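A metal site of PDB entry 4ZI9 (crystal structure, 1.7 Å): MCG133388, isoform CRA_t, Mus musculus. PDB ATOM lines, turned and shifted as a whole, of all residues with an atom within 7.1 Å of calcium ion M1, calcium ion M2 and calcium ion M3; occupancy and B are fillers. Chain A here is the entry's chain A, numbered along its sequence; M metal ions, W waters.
Within 4 Å of calcium ion M1: Glu 117, Glu 176, Asp 207, Val 208, Asp 210, Asn 211 and Asp 243.
The nearest printed residue that does not touch calcium ion M1 is Arg 175 (4.4 Å).
Calcium ion M1 is bound by the side-chain carboxylate (OD1) of Asp 207 (2.3 Å), the side-chain carboxylate (OE2) of Glu 176 (2.3 Å), the side-chain carboxylate (OE1) of Glu 117 (2.3 Å), the side-chain carboxylate (OD1) of Asp 210 (2.3 Å), the side-chain carboxylate (OD1) of Asp 243 (2.4 Å), the backbone carbonyl oxygen (O) of Val 208 (2.5 Å) and the side-chain carboxylate (OE1) of Glu 176 (2.6 Å).
The side-chain carboxylate (OE1) of Glu 176 lies close to the side-chain amide nitrogen (ND2) of Asn 211, 3.4 Å away.
The side-chain carboxylate (OE2) of Glu 176 lies close to the guanidinium group (NH2) of Arg 175.
The side-chain amide nitrogen (ND2) of Asn 247 sits at hydrogen-bond distance from the side-chain carboxylate (OD2) of Asp 207, at 2.7 Å.
NE of Arg 175 sits close to OD1 of Asp 207 (3.2 Å).
The side-chain carboxylate (OD2) of Asp 207 is in hydrogen-bond range of the backbone NH (N) of Glu 244 (3.0 Å).
The backbone carbonyl oxygen of Val 206 lies within hydrogen-bond range of the backbone NH of Glu 117 (2.9 Å).
ND2 of Asn 209 sits at hydrogen-bond distance from O of Ala 298 (3.2 Å).
The side-chain carboxylate (OD1) of Asp 296 is in hydrogen-bond range of the backbone NH (N) of Ala 298 (2.8 Å).
Calcium ion M2 is bound by the backbone carbonyl oxygen (O) of Asn 247 (2.3 Å), the backbone carbonyl oxygen (O) of Asn 211 (2.3 Å), the side-chain amide oxygen (OD1) of Asn 209 (2.3 Å), the side-chain carboxylate (OD2) of Asp 243 (2.4 Å), the side-chain carboxylate (OD2) of Asp 241 (2.5 Å), the side-chain carboxylate (OD2) of Asp 296 (2.6 Å) and the side-chain carboxylate (OD1) of Asp 241 (2.6 Å).
Along chain A the residues within 4 Å of calcium ion M2 span positions 209 to 296.
Calcium ion M3 is bound by OE1 of Glu 176 (2.3 Å), OD1 of Asp 174 (2.3 Å), water W2 (2.4 Å), OE2 of Glu 117 (2.4 Å), water W1 (2.5 Å) and OD2 of Asp 210 (2.5 Å).
Along chain A the residues within 4 Å of calcium ion M3 span positions 117 to 210.
The nearest printed residue that does not touch calcium ion M3 is Asn 211 (4.2 Å).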
ATOM      1  N   GLU A 117     -20.384  19.862 -13.199  1.00  0.00           N
ATOM      2  CA  GLU A 117     -19.032  20.403 -13.215  1.00  0.00           C
ATOM      3  C   GLU A 117     -18.864  21.565 -12.242  1.00  0.00           C
ATOM      4  O   GLU A 117     -17.717  21.926 -11.904  1.00  0.00           O
ATOM      5  CB  GLU A 117     -18.625  20.810 -14.630  1.00  0.00           C
ATOM      6  CG  GLU A 117     -19.563  21.791 -15.328  1.00  0.00           C
ATOM      7  CD  GLU A 117     -19.019  22.201 -16.670  1.00  0.00           C
ATOM      8  OE1 GLU A 117     -19.822  22.451 -17.584  1.00  0.00           O
ATOM      9  OE2 GLU A 117     -17.777  22.260 -16.799  1.00  0.00           O
ATOM     10  N   LEU A 173     -14.140  20.193 -11.055  1.00  0.00           N
ATOM     11  CA  LEU A 173     -14.393  19.485 -12.297  1.00  0.00           C
ATOM     12  C   LEU A 173     -14.575  20.440 -13.484  1.00  0.00           C
ATOM     13  O   LEU A 173     -14.828  21.635 -13.301  1.00  0.00           O
ATOM     14  CB  LEU A 173     -15.633  18.618 -12.142  1.00  0.00           C
ATOM     15  CG  LEU A 173     -15.558  17.623 -10.981  1.00  0.00           C
ATOM     16  CD1 LEU A 173     -16.912  16.968 -10.844  1.00  0.00           C
ATOM     17  CD2 LEU A 173     -14.468  16.588 -11.261  1.00  0.00           C
ATOM     18  N   ASP A 174     -14.433  19.912 -14.707  1.00  0.00           N
ATOM     19  CA  ASP A 174     -14.671  20.701 -15.925  1.00  0.00           C
ATOM     20  C   ASP A 174     -15.025  19.766 -17.060  1.00  0.00           C
ATOM     21  O   ASP A 174     -14.156  19.093 -17.606  1.00  0.00           O
ATOM     22  CB  ASP A 174     -13.458  21.547 -16.297  1.00  0.00           C
ATOM     23  CG  ASP A 174     -13.650  22.316 -17.604  1.00  0.00           C
ATOM     24  OD1 ASP A 174     -14.766  22.383 -18.161  1.00  0.00           O
ATOM     25  OD2 ASP A 174     -12.656  22.875 -18.099  1.00  0.00           O
ATOM     26  N   ARG A 175     -16.310  19.687 -17.401  1.00  0.00           N
ATOM     27  CA  ARG A 175     -16.762  18.793 -18.468  1.00  0.00           C
ATOM     28  C   ARG A 175     -16.079  19.081 -19.808  1.00  0.00           C
ATOM     29  O   ARG A 175     -15.888  18.171 -20.597  1.00  0.00           O
ATOM     30  CB  ARG A 175     -18.274  18.904 -18.624  1.00  0.00           C
ATOM     31  CG  ARG A 175     -18.934  17.750 -19.359  1.00  0.00           C
ATOM     32  CD  ARG A 175     -20.184  18.227 -20.056  1.00  0.00           C
ATOM     33  NE  ARG A 175     -19.834  19.238 -21.063  1.00  0.00           N
ATOM     34  CZ  ARG A 175     -19.556  18.964 -22.330  1.00  0.00           C
ATOM     35  NH1 ARG A 175     -19.638  17.711 -22.780  1.00  0.00           N
ATOM     36  NH2 ARG A 175     -19.218  19.929 -23.163  1.00  0.00           N
ATOM     37  N   GLU A 176     -15.715  20.340 -20.068  1.00  0.00           N
ATOM     38  CA  GLU A 176     -15.053  20.661 -21.327  1.00  0.00           C
ATOM     39  C   GLU A 176     -13.593  20.159 -21.367  1.00  0.00           C
ATOM     40  O   GLU A 176     -12.980  20.128 -22.428  1.00  0.00           O
ATOM     41  CB  GLU A 176     -15.092  22.176 -21.593  1.00  0.00           C
ATOM     42  CG  GLU A 176     -16.435  22.674 -22.053  1.00  0.00           C
ATOM     43  CD  GLU A 176     -17.509  22.668 -20.957  1.00  0.00           C
ATOM     44  OE1 GLU A 176     -17.253  23.163 -19.831  1.00  0.00           O
ATOM     45  OE2 GLU A 176     -18.640  22.221 -21.246  1.00  0.00           O
ATOM     46  N   LYS A 177     -13.063  19.740 -20.225  1.00  0.00           N
ATOM     47  CA  LYS A 177     -11.738  19.088 -20.194  1.00  0.00           C
ATOM     48  C   LYS A 177     -11.917  17.577 -20.085  1.00  0.00           C
ATOM     49  O   LYS A 177     -11.391  16.818 -20.884  1.00  0.00           O
ATOM     50  CB  LYS A 177     -10.899  19.619 -19.025  1.00  0.00           C
ATOM     51  CG  LYS A 177      -9.482  19.048 -18.924  1.00  0.00           C
ATOM     52  CD  LYS A 177      -8.767  19.529 -17.648  1.00  0.00           C
ATOM     53  CE  LYS A 177      -7.241  19.360 -17.718  1.00  0.00           C
ATOM     54  NZ  LYS A 177      -6.802  17.940 -17.780  1.00  0.00           N
ATOM     55  N   VAL A 206     -21.678  16.447 -15.307  1.00  0.00           N
ATOM     56  CA  VAL A 206     -22.865  17.052 -15.890  1.00  0.00           C
ATOM     57  C   VAL A 206     -22.571  18.494 -16.324  1.00  0.00           C
ATOM     58  O   VAL A 206     -21.907  19.269 -15.620  1.00  0.00           O
ATOM     59  CB  VAL A 206     -24.048  17.005 -14.915  1.00  0.00           C
ATOM     60  CG1 VAL A 206     -25.269  17.568 -15.569  1.00  0.00           C
ATOM     61  CG2 VAL A 206     -24.315  15.571 -14.527  1.00  0.00           C
ATOM     62  N   ASP A 207     -23.023  18.825 -17.523  1.00  0.00           N
ATOM     63  CA  ASP A 207     -22.694  20.120 -18.116  1.00  0.00           C
ATOM     64  C   ASP A 207     -23.325  21.295 -17.366  1.00  0.00           C
ATOM     65  O   ASP A 207     -24.446  21.179 -16.854  1.00  0.00           O
ATOM     66  CB  ASP A 207     -23.127  20.151 -19.594  1.00  0.00           C
ATOM     67  CG  ASP A 207     -22.628  21.405 -20.340  1.00  0.00           C
ATOM     68  OD1 ASP A 207     -21.469  21.833 -20.155  1.00  0.00           O
ATOM     69  OD2 ASP A 207     -23.417  21.974 -21.098  1.00  0.00           O
ATOM     70  N   VAL A 208     -22.588  22.394 -17.284  1.00  0.00           N
ATOM     71  CA  VAL A 208     -23.152  23.706 -16.927  1.00  0.00           C
ATOM     72  C   VAL A 208     -22.893  24.657 -18.103  1.00  0.00           C
ATOM     73  O   VAL A 208     -21.860  24.537 -18.775  1.00  0.00           O
ATOM     74  CB  VAL A 208     -22.518  24.256 -15.631  1.00  0.00           C
ATOM     75  CG1 VAL A 208     -22.949  25.705 -15.370  1.00  0.00           C
ATOM     76  CG2 VAL A 208     -22.875  23.349 -14.429  1.00  0.00           C
ATOM     77  N   ASN A 209     -23.808  25.599 -18.371  1.00  0.00           N
ATOM     78  CA  ASN A 209     -23.524  26.570 -19.424  1.00  0.00           C
ATOM     79  C   ASN A 209     -22.504  27.552 -18.887  1.00  0.00           C
ATOM     80  O   ASN A 209     -22.880  28.607 -18.385  1.00  0.00           O
ATOM     81  CB  ASN A 209     -24.771  27.312 -19.880  1.00  0.00           C
ATOM     82  CG  ASN A 209     -24.518  28.090 -21.175  1.00  0.00           C
ATOM     83  OD1 ASN A 209     -23.666  27.686 -22.006  1.00  0.00           O
ATOM     84  ND2 ASN A 209     -25.222  29.211 -21.353  1.00  0.00           N
ATOM     85  N   ASP A 210     -21.238  27.220 -18.988  1.00  0.00           N
ATOM     86  CA  ASP A 210     -20.220  28.094 -18.412  1.00  0.00           C
ATOM     87  C   ASP A 210     -19.230  28.630 -19.450  1.00  0.00           C
ATOM     88  O   ASP A 210     -18.160  29.149 -19.097  1.00  0.00           O
ATOM     89  CB  ASP A 210     -19.491  27.399 -17.244  1.00  0.00           C
ATOM     90  CG  ASP A 210     -18.832  26.067 -17.623  1.00  0.00           C
ATOM     91  OD1 ASP A 210     -19.211  25.407 -18.624  1.00  0.00           O
ATOM     92  OD2 ASP A 210     -17.915  25.662 -16.879  1.00  0.00           O
ATOM     93  N   ASN A 211     -19.578  28.508 -20.724  1.00  0.00           N
ATOM     94  CA  ASN A 211     -18.790  29.124 -21.793  1.00  0.00           C
ATOM     95  C   ASN A 211     -19.709  29.921 -22.694  1.00  0.00           C
ATOM     96  O   ASN A 211     -20.731  29.405 -23.140  1.00  0.00           O
ATOM     97  CB  ASN A 211     -18.053  28.106 -22.654  1.00  0.00           C
ATOM     98  CG  ASN A 211     -17.032  27.309 -21.881  1.00  0.00           C
ATOM     99  OD1 ASN A 211     -15.856  27.656 -21.848  1.00  0.00           O
ATOM    100  ND2 ASN A 211     -17.486  26.234 -21.237  1.00  0.00           N
ATOM    101  N   PRO A 212     -19.352  31.175 -22.959  1.00  0.00           N
ATOM    102  CA  PRO A 212     -20.061  31.930 -23.992  1.00  0.00           C
ATOM    103  C   PRO A 212     -19.640  31.463 -25.382  1.00  0.00           C
ATOM    104  O   PRO A 212     -18.578  30.896 -25.553  1.00  0.00           O
ATOM    105  CB  PRO A 212     -19.610  33.364 -23.745  1.00  0.00           C
ATOM    106  CG  PRO A 212     -18.170  33.174 -23.337  1.00  0.00           C
ATOM    107  CD  PRO A 212     -18.185  31.920 -22.450  1.00  0.00           C
ATOM    108  N   PRO A 213     -20.477  31.726 -26.395  1.00  0.00           N
ATOM    109  CA  PRO A 213     -19.965  31.482 -27.753  1.00  0.00           C
ATOM    110  C   PRO A 213     -18.751  32.383 -28.057  1.00  0.00           C
ATOM    111  O   PRO A 213     -18.449  33.311 -27.312  1.00  0.00           O
ATOM    112  CB  PRO A 213     -21.148  31.833 -28.653  1.00  0.00           C
ATOM    113  CG  PRO A 213     -22.342  31.946 -27.742  1.00  0.00           C
ATOM    114  CD  PRO A 213     -21.829  32.288 -26.386  1.00  0.00           C
ATOM    115  N   THR A 240     -18.390  29.498 -32.242  1.00  0.00           N
ATOM    116  CA  THR A 240     -18.343  28.150 -31.679  1.00  0.00           C
ATOM    117  C   THR A 240     -18.614  28.239 -30.184  1.00  0.00           C
ATOM    118  O   THR A 240     -18.472  29.307 -29.582  1.00  0.00           O
ATOM    119  CB  THR A 240     -16.995  27.493 -31.933  1.00  0.00           C
ATOM    120  OG1 THR A 240     -15.945  28.321 -31.424  1.00  0.00           O
ATOM    121  CG2 THR A 240     -16.777  27.287 -33.428  1.00  0.00           C
ATOM    122  N   ASP A 241     -19.008  27.114 -29.583  1.00  0.00           N
ATOM    123  CA  ASP A 241     -19.380  27.080 -28.169  1.00  0.00           C
ATOM    124  C   ASP A 241     -19.167  25.649 -27.657  1.00  0.00           C
ATOM    125  O   ASP A 241     -19.770  24.717 -28.176  1.00  0.00           O
ATOM    126  CB  ASP A 241     -20.812  27.508 -27.967  1.00  0.00           C
ATOM    127  CG  ASP A 241     -21.173  27.710 -26.497  1.00  0.00           C
ATOM    128  OD1 ASP A 241     -20.772  26.888 -25.626  1.00  0.00           O
ATOM    129  OD2 ASP A 241     -21.856  28.716 -26.213  1.00  0.00           O
ATOM    130  N   PRO A 242     -18.291  25.479 -26.663  1.00  0.00           N
ATOM    131  CA  PRO A 242     -17.843  24.138 -26.257  1.00  0.00           C
ATOM    132  C   PRO A 242     -18.772  23.429 -25.256  1.00  0.00           C
ATOM    133  O   PRO A 242     -18.507  22.292 -24.897  1.00  0.00           O
ATOM    134  CB  PRO A 242     -16.485  24.421 -25.628  1.00  0.00           C
ATOM    135  CG  PRO A 242     -16.632  25.801 -25.071  1.00  0.00           C
ATOM    136  CD  PRO A 242     -17.545  26.550 -25.980  1.00  0.00           C
ATOM    137  N   ASP A 243     -19.824  24.088 -24.806  1.00  0.00           N
ATOM    138  CA  ASP A 243     -20.767  23.443 -23.900  1.00  0.00           C
ATOM    139  C   ASP A 243     -21.613  22.416 -24.652  1.00  0.00           C
ATOM    140  O   ASP A 243     -21.562  22.334 -25.894  1.00  0.00           O
ATOM    141  CB  ASP A 243     -21.669  24.484 -23.211  1.00  0.00           C
ATOM    142  CG  ASP A 243     -20.890  25.415 -22.317  1.00  0.00           C
ATOM    143  OD1 ASP A 243     -20.048  24.944 -21.526  1.00  0.00           O
ATOM    144  OD2 ASP A 243     -21.084  26.623 -22.448  1.00  0.00           O
ATOM    145  N   GLU A 244     -22.401  21.646 -23.903  1.00  0.00           N
ATOM    146  CA  GLU A 244     -23.119  20.485 -24.432  1.00  0.00           C
ATOM    147  C   GLU A 244     -24.567  20.805 -24.801  1.00  0.00           C
ATOM    148  O   GLU A 244     -25.257  21.535 -24.092  1.00  0.00           O
ATOM    149  CB  GLU A 244     -23.092  19.343 -23.406  1.00  0.00           C
ATOM    150  CG  GLU A 244     -23.832  18.077 -23.833  1.00  0.00           C
ATOM    151  CD  GLU A 244     -23.740  16.947 -22.796  1.00  0.00           C
ATOM    152  OE1 GLU A 244     -23.554  17.251 -21.599  1.00  0.00           O
ATOM    153  OE2 GLU A 244     -23.831  15.769 -23.180  1.00  0.00           O
ATOM    154  N   ALA A 246     -27.983  22.198 -25.945  1.00  0.00           N
ATOM    155  CA  ALA A 246     -28.508  23.550 -26.072  1.00  0.00           C
ATOM    156  C   ALA A 246     -27.532  24.604 -25.551  1.00  0.00           C
ATOM    157  O   ALA A 246     -27.515  25.733 -26.057  1.00  0.00           O
ATOM    158  CB  ALA A 246     -29.823  23.663 -25.356  1.00  0.00           C
ATOM    159  N   ASN A 247     -26.752  24.242 -24.547  1.00  0.00           N
ATOM    160  CA  ASN A 247     -25.746  25.160 -23.993  1.00  0.00           C
ATOM    161  C   ASN A 247     -24.651  25.561 -24.988  1.00  0.00           C
ATOM    162  O   ASN A 247     -24.013  26.609 -24.816  1.00  0.00           O
ATOM    163  CB  ASN A 247     -25.104  24.547 -22.747  1.00  0.00           C
ATOM    164  CG  ASN A 247     -26.104  24.270 -21.664  1.00  0.00           C
ATOM    165  OD1 ASN A 247     -27.140  24.925 -21.586  1.00  0.00           O
ATOM    166  ND2 ASN A 247     -25.795  23.309 -20.795  1.00  0.00           N
ATOM    167  N   GLY A 248     -24.432  24.723 -25.998  1.00  0.00           N
ATOM    168  CA  GLY A 248     -23.423  24.962 -27.024  1.00  0.00           C
ATOM    169  C   GLY A 248     -24.006  25.273 -28.408  1.00  0.00           C
ATOM    170  O   GLY A 248     -23.274  25.389 -29.395  1.00  0.00           O
ATOM    171  N   ARG A 249     -25.326  25.372 -28.478  1.00  0.00           N
ATOM    172  CA  ARG A 249     -26.006  25.644 -29.748  1.00  0.00           C
ATOM    173  C   ARG A 249     -26.223  27.145 -29.921  1.00  0.00           C
ATOM    174  O   ARG A 249     -26.885  27.788 -29.099  1.00  0.00           O
ATOM    175  CB  ARG A 249     -27.351  24.899 -29.780  1.00  0.00           C
ATOM    176  CG  ARG A 249     -28.127  24.982 -31.081  1.00  0.00           C
ATOM    177  CD  ARG A 249     -29.209  23.904 -31.073  1.00  0.00           C
ATOM    178  NE  ARG A 249     -28.678  22.606 -30.648  1.00  0.00           N
ATOM    179  CZ  ARG A 249     -29.127  21.891 -29.614  1.00  0.00           C
ATOM    180  NH1 ARG A 249     -30.133  22.338 -28.871  1.00  0.00           N
ATOM    181  NH2 ARG A 249     -28.562  20.718 -29.327  1.00  0.00           N
ATOM    182  N   VAL A 250     -25.666  27.714 -30.986  1.00  0.00           N
ATOM    183  CA  VAL A 250     -25.690  29.168 -31.104  1.00  0.00           C
ATOM    184  C   VAL A 250     -26.525  29.676 -32.272  1.00  0.00           C
ATOM    185  O   VAL A 250     -26.574  29.083 -33.359  1.00  0.00           O
ATOM    186  CB  VAL A 250     -24.248  29.740 -31.198  1.00  0.00           C
ATOM    187  CG1 VAL A 250     -23.225  28.676 -30.887  1.00  0.00           C
ATOM    188  CG2 VAL A 250     -23.976  30.383 -32.522  1.00  0.00           C
ATOM    189  N   ASP A 296     -25.956  31.457 -27.191  1.00  0.00           N
ATOM    190  CA  ASP A 296     -26.147  30.014 -27.004  1.00  0.00           C
ATOM    191  C   ASP A 296     -27.581  29.800 -26.503  1.00  0.00           C
ATOM    192  O   ASP A 296     -28.370  30.725 -26.448  1.00  0.00           O
ATOM    193  CB  ASP A 296     -25.110  29.389 -26.049  1.00  0.00           C
ATOM    194  CG  ASP A 296     -25.170  29.941 -24.630  1.00  0.00           C
ATOM    195  OD1 ASP A 296     -26.234  30.420 -24.144  1.00  0.00           O
ATOM    196  OD2 ASP A 296     -24.107  29.865 -23.969  1.00  0.00           O
ATOM    197  N   GLY A 297     -27.909  28.572 -26.126  1.00  0.00           N
ATOM    198  CA  GLY A 297     -29.289  28.302 -25.792  1.00  0.00           C
ATOM    199  C   GLY A 297     -29.652  28.613 -24.353  1.00  0.00           C
ATOM    200  O   GLY A 297     -30.763  28.309 -23.929  1.00  0.00           O
ATOM    201  N   ALA A 298     -28.742  29.236 -23.602  1.00  0.00           N
ATOM    202  CA  ALA A 298     -28.988  29.418 -22.164  1.00  0.00           C
ATOM    203  C   ALA A 298     -28.405  30.720 -21.599  1.00  0.00           C
ATOM    204  O   ALA A 298     -27.881  30.723 -20.479  1.00  0.00           O
ATOM    205  CB  ALA A 298     -28.448  28.198 -21.366  1.00  0.00           C
ATOM    206  N   LEU A 300     -25.869  32.965 -22.606  1.00  0.00           N
ATOM    207  CA  LEU A 300     -24.543  33.541 -22.772  1.00  0.00           C
ATOM    208  C   LEU A 300     -24.415  34.005 -24.224  1.00  0.00           C
ATOM    209  O   LEU A 300     -25.080  33.503 -25.120  1.00  0.00           O
ATOM    210  CB  LEU A 300     -23.434  32.553 -22.395  1.00  0.00           C
ATOM    211  CG  LEU A 300     -23.360  32.168 -20.913  1.00  0.00           C
ATOM    212  CD1 LEU A 300     -22.220  31.210 -20.705  1.00  0.00           C
ATOM    213  CD2 LEU A 300     -23.182  33.417 -20.049  1.00  0.00           C
HETATM  214 CA    CA M   1     -19.879  23.427 -19.698  1.00  0.00          CA
HETATM  215 CA    CA M   2     -22.380  27.977 -23.930  1.00  0.00          CA
HETATM  216 CA    CA M   3     -16.437  23.930 -17.850  1.00  0.00          CA
HETATM  217  O   HOH W   1     -15.412  25.850 -18.992  1.00  0.00           O
HETATM  218  O   HOH W   2     -15.273  24.495 -15.885  1.00  0.00           O
